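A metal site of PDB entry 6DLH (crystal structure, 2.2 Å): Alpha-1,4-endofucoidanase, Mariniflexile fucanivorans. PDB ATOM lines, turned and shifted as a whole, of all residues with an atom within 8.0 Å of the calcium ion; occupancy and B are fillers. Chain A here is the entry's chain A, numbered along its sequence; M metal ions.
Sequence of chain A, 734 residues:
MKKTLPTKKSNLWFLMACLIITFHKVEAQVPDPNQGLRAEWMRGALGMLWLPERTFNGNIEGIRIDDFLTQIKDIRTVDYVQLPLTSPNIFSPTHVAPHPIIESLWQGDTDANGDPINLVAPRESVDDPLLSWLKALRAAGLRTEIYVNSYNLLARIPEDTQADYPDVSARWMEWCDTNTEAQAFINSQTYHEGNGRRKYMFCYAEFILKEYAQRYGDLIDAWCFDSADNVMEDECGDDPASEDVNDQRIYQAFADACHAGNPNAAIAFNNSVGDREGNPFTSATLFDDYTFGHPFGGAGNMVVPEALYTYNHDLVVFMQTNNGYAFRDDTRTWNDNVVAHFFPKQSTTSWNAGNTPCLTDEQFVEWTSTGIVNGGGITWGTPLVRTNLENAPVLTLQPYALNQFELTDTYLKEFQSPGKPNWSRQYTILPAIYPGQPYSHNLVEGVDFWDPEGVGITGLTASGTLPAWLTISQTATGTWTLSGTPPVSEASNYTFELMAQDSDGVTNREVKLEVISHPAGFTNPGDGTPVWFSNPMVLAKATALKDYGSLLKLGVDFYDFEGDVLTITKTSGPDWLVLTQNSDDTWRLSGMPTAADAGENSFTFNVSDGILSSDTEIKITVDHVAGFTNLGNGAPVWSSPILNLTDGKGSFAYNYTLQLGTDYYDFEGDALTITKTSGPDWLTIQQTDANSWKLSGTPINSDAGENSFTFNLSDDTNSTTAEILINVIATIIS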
ATOM      1  N   ASN A 633     -25.005  14.908 -15.394  1.00  0.00           N
ATOM      2  CA  ASN A 633     -23.848  14.130 -14.971  1.00  0.00           C
ATOM      3  C   ASN A 633     -22.614  15.017 -14.764  1.00  0.00           C
ATOM      4  O   ASN A 633     -21.546  14.514 -14.399  1.00  0.00           O
ATOM      5  CB  ASN A 633     -23.578  12.946 -15.908  1.00  0.00           C
ATOM      6  CG  ASN A 633     -23.379  13.349 -17.353  1.00  0.00           C
ATOM      7  OD1 ASN A 633     -22.255  13.511 -17.798  1.00  0.00           O
ATOM      8  ND2 ASN A 633     -24.472  13.516 -18.082  1.00  0.00           N
ATOM      9  N   GLY A 634     -22.761  16.313 -15.016  1.00  0.00           N
ATOM     10  CA  GLY A 634     -21.703  17.270 -14.729  1.00  0.00           C
ATOM     11  C   GLY A 634     -20.970  17.751 -15.982  1.00  0.00           C
ATOM     12  O   GLY A 634     -20.132  18.650 -15.899  1.00  0.00           O
ATOM     13  N   ALA A 635     -21.313  17.137 -17.127  1.00  0.00           N
ATOM     14  CA  ALA A 635     -20.704  17.473 -18.408  1.00  0.00           C
ATOM     15  C   ALA A 635     -21.134  18.864 -18.846  1.00  0.00           C
ATOM     16  O   ALA A 635     -22.280  19.250 -18.644  1.00  0.00           O
ATOM     17  CB  ALA A 635     -21.100  16.442 -19.431  1.00  0.00           C
ATOM     18  N   PRO A 636     -20.215  19.688 -19.410  1.00  0.00           N
ATOM     19  CA  PRO A 636     -20.587  20.839 -20.242  1.00  0.00           C
ATOM     20  C   PRO A 636     -21.366  20.404 -21.480  1.00  0.00           C
ATOM     21  O   PRO A 636     -21.345  19.221 -21.816  1.00  0.00           O
ATOM     22  CB  PRO A 636     -19.235  21.467 -20.611  1.00  0.00           C
ATOM     23  CG  PRO A 636     -18.288  20.994 -19.533  1.00  0.00           C
ATOM     24  CD  PRO A 636     -18.752  19.583 -19.223  1.00  0.00           C
ATOM     25  N   TYR A 665     -21.854  26.034 -21.777  1.00  0.00           N
ATOM     26  CA  TYR A 665     -22.280  26.198 -20.399  1.00  0.00           C
ATOM     27  C   TYR A 665     -21.918  24.968 -19.576  1.00  0.00           C
ATOM     28  O   TYR A 665     -22.028  23.842 -20.042  1.00  0.00           O
ATOM     29  CB  TYR A 665     -23.801  26.424 -20.373  1.00  0.00           C
ATOM     30  CG  TYR A 665     -24.353  26.959 -19.073  1.00  0.00           C
ATOM     31  CD1 TYR A 665     -23.891  28.154 -18.541  1.00  0.00           C
ATOM     32  CD2 TYR A 665     -25.355  26.290 -18.398  1.00  0.00           C
ATOM     33  CE1 TYR A 665     -24.417  28.667 -17.365  1.00  0.00           C
ATOM     34  CE2 TYR A 665     -25.894  26.787 -17.215  1.00  0.00           C
ATOM     35  CZ  TYR A 665     -25.415  27.982 -16.708  1.00  0.00           C
ATOM     36  OH  TYR A 665     -25.937  28.479 -15.549  1.00  0.00           O
ATOM     37  N   ASP A 666     -21.509  25.212 -18.320  1.00  0.00           N
ATOM     38  CA  ASP A 666     -21.239  24.156 -17.355  1.00  0.00           C
ATOM     39  C   ASP A 666     -22.091  24.371 -16.114  1.00  0.00           C
ATOM     40  O   ASP A 666     -21.895  25.340 -15.388  1.00  0.00           O
ATOM     41  CB  ASP A 666     -19.748  24.081 -17.019  1.00  0.00           C
ATOM     42  CG  ASP A 666     -19.445  23.044 -15.953  1.00  0.00           C
ATOM     43  OD1 ASP A 666     -19.611  21.839 -16.244  1.00  0.00           O
ATOM     44  OD2 ASP A 666     -19.076  23.441 -14.825  1.00  0.00           O
ATOM     45  N   PHE A 667     -22.979  23.409 -15.830  1.00  0.00           N
ATOM     46  CA  PHE A 667     -23.993  23.544 -14.791  1.00  0.00           C
ATOM     47  C   PHE A 667     -23.403  23.572 -13.381  1.00  0.00           C
ATOM     48  O   PHE A 667     -24.143  23.757 -12.423  1.00  0.00           O
ATOM     49  CB  PHE A 667     -25.067  22.473 -14.958  1.00  0.00           C
ATOM     50  CG  PHE A 667     -26.012  22.739 -16.110  1.00  0.00           C
ATOM     51  CD1 PHE A 667     -27.163  23.509 -15.913  1.00  0.00           C
ATOM     52  CD2 PHE A 667     -25.761  22.242 -17.375  1.00  0.00           C
ATOM     53  CE1 PHE A 667     -28.032  23.757 -16.964  1.00  0.00           C
ATOM     54  CE2 PHE A 667     -26.623  22.497 -18.424  1.00  0.00           C
ATOM     55  CZ  PHE A 667     -27.766  23.257 -18.222  1.00  0.00           C
ATOM     56  N   GLU A 668     -22.074  23.417 -13.246  1.00  0.00           N
ATOM     57  CA  GLU A 668     -21.451  23.457 -11.936  1.00  0.00           C
ATOM     58  C   GLU A 668     -20.494  24.634 -11.836  1.00  0.00           C
ATOM     59  O   GLU A 668     -19.947  24.911 -10.776  1.00  0.00           O
ATOM     60  CB  GLU A 668     -20.764  22.124 -11.594  1.00  0.00           C
ATOM     61  CG  GLU A 668     -21.693  20.921 -11.578  1.00  0.00           C
ATOM     62  CD  GLU A 668     -22.048  20.387 -12.963  1.00  0.00           C
ATOM     63  OE1 GLU A 668     -21.279  20.651 -13.906  1.00  0.00           O
ATOM     64  OE2 GLU A 668     -23.097  19.718 -13.090  1.00  0.00           O
ATOM     65  N   GLY A 669     -20.315  25.343 -12.966  1.00  0.00           N
ATOM     66  CA  GLY A 669     -19.470  26.527 -13.008  1.00  0.00           C
ATOM     67  C   GLY A 669     -17.990  26.202 -12.849  1.00  0.00           C
ATOM     68  O   GLY A 669     -17.233  27.017 -12.338  1.00  0.00           O
ATOM     69  N   ASP A 670     -17.603  24.998 -13.300  1.00  0.00           N
ATOM     70  CA  ASP A 670     -16.211  24.584 -13.337  1.00  0.00           C
ATOM     71  C   ASP A 670     -15.485  25.412 -14.403  1.00  0.00           C
ATOM     72  O   ASP A 670     -16.099  25.829 -15.385  1.00  0.00           O
ATOM     73  CB  ASP A 670     -16.068  23.096 -13.666  1.00  0.00           C
ATOM     74  CG  ASP A 670     -16.811  22.170 -12.715  1.00  0.00           C
ATOM     75  OD1 ASP A 670     -16.747  22.411 -11.500  1.00  0.00           O
ATOM     76  OD2 ASP A 670     -17.462  21.211 -13.216  1.00  0.00           O
ATOM     77  N   ALA A 671     -14.181  25.631 -14.187  1.00  0.00           N
ATOM     78  CA  ALA A 671     -13.307  26.152 -15.229  1.00  0.00           C
ATOM     79  C   ALA A 671     -13.338  25.192 -16.428  1.00  0.00           C
ATOM     80  O   ALA A 671     -13.302  23.979 -16.243  1.00  0.00           O
ATOM     81  CB  ALA A 671     -11.920  26.329 -14.672  1.00  0.00           C
ATOM     82  N   LEU A 672     -13.443  25.754 -17.635  1.00  0.00           N
ATOM     83  CA  LEU A 672     -13.544  24.944 -18.848  1.00  0.00           C
ATOM     84  C   LEU A 672     -12.283  25.117 -19.683  1.00  0.00           C
ATOM     85  O   LEU A 672     -11.599  26.138 -19.601  1.00  0.00           O
ATOM     86  CB  LEU A 672     -14.781  25.363 -19.656  1.00  0.00           C
ATOM     87  CG  LEU A 672     -16.153  25.031 -19.086  1.00  0.00           C
ATOM     88  CD1 LEU A 672     -16.110  23.841 -18.126  1.00  0.00           C
ATOM     89  CD2 LEU A 672     -16.778  26.238 -18.406  1.00  0.00           C
ATOM     90  N   SER A 714     -14.062  20.310 -21.680  1.00  0.00           N
ATOM     91  CA  SER A 714     -13.645  19.176 -20.882  1.00  0.00           C
ATOM     92  C   SER A 714     -13.838  19.317 -19.368  1.00  0.00           C
ATOM     93  O   SER A 714     -13.935  18.302 -18.684  1.00  0.00           O
ATOM     94  CB  SER A 714     -12.228  18.759 -21.209  1.00  0.00           C
ATOM     95  OG  SER A 714     -11.278  19.578 -20.544  1.00  0.00           O
ATOM     96  N   ASP A 715     -13.851  20.545 -18.839  1.00  0.00           N
ATOM     97  CA  ASP A 715     -13.725  20.775 -17.398  1.00  0.00           C
ATOM     98  C   ASP A 715     -12.606  19.915 -16.816  1.00  0.00           C
ATOM     99  O   ASP A 715     -11.487  19.910 -17.339  1.00  0.00           O
ATOM    100  CB  ASP A 715     -15.070  20.786 -16.659  1.00  0.00           C
ATOM    101  CG  ASP A 715     -15.699  19.448 -16.279  1.00  0.00           C
ATOM    102  OD1 ASP A 715     -14.970  18.439 -16.228  1.00  0.00           O
ATOM    103  OD2 ASP A 715     -16.914  19.429 -16.001  1.00  0.00           O
ATOM    104  N   ASP A 716     -12.894  19.188 -15.730  1.00  0.00           N
ATOM    105  CA  ASP A 716     -11.899  18.375 -15.042  1.00  0.00           C
ATOM    106  C   ASP A 716     -12.046  16.900 -15.425  1.00  0.00           C
ATOM    107  O   ASP A 716     -11.043  16.195 -15.537  1.00  0.00           O
ATOM    108  CB  ASP A 716     -11.946  18.561 -13.523  1.00  0.00           C
ATOM    109  CG  ASP A 716     -10.893  19.501 -12.979  1.00  0.00           C
ATOM    110  OD1 ASP A 716      -9.853  19.684 -13.652  1.00  0.00           O
ATOM    111  OD2 ASP A 716     -11.099  20.038 -11.869  1.00  0.00           O
ATOM    112  N   THR A 717     -13.280  16.433 -15.613  1.00  0.00           N
ATOM    113  CA  THR A 717     -13.537  15.005 -15.739  1.00  0.00           C
ATOM    114  C   THR A 717     -14.351  14.696 -16.996  1.00  0.00           C
ATOM    115  O   THR A 717     -13.922  13.895 -17.825  1.00  0.00           O
ATOM    116  CB  THR A 717     -14.145  14.415 -14.454  1.00  0.00           C
ATOM    117  OG1 THR A 717     -15.535  14.754 -14.360  1.00  0.00           O
ATOM    118  CG2 THR A 717     -13.425  14.851 -13.183  1.00  0.00           C
ATOM    119  N   ASN A 718     -15.520  15.332 -17.113  1.00  0.00           N
ATOM    120  CA  ASN A 718     -16.441  15.070 -18.212  1.00  0.00           C
ATOM    121  C   ASN A 718     -16.133  16.010 -19.379  1.00  0.00           C
ATOM    122  O   ASN A 718     -15.931  17.203 -19.164  1.00  0.00           O
ATOM    123  CB  ASN A 718     -17.901  15.230 -17.764  1.00  0.00           C
ATOM    124  CG  ASN A 718     -18.535  13.921 -17.339  1.00  0.00           C
ATOM    125  OD1 ASN A 718     -19.008  13.799 -16.213  1.00  0.00           O
ATOM    126  ND2 ASN A 718     -18.554  12.948 -18.238  1.00  0.00           N
ATOM    127  N   SER A 719     -16.127  15.467 -20.599  1.00  0.00           N
ATOM    128  CA  SER A 719     -15.873  16.243 -21.802  1.00  0.00           C
ATOM    129  C   SER A 719     -16.981  16.001 -22.827  1.00  0.00           C
ATOM    130  O   SER A 719     -17.450  14.878 -22.977  1.00  0.00           O
ATOM    131  CB  SER A 719     -14.514  15.914 -22.378  1.00  0.00           C
HETATM  132 CA    CA M   1     -18.701  20.097 -14.665  1.00  0.00          CA
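Of the 18 residues printed, 5 come within 4 Å of the calcium ion.
The calcium ion is bound by the side-chain carboxylate (OD2) of Asp 670, the side-chain carboxylate (OD2) of Asp 715, the backbone carbonyl oxygen (O) of Gly 634, the side-chain carboxylate (OD1) of Asp 666 and the side-chain carboxylate (OE1) of Glu 668. The calcium ion has five donor atoms within binding distance.
OD1 of Asp 715 sits at hydrogen-bond distance from N of Asn 718, at 3.3 Å. N of Thr 717 is in hydrogen-bond range of OD1 of Asp 715, at 2.7 Å. OD2 of Asp 666 sits at hydrogen-bond distance from N of Gly 669, at 2.9 Å.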
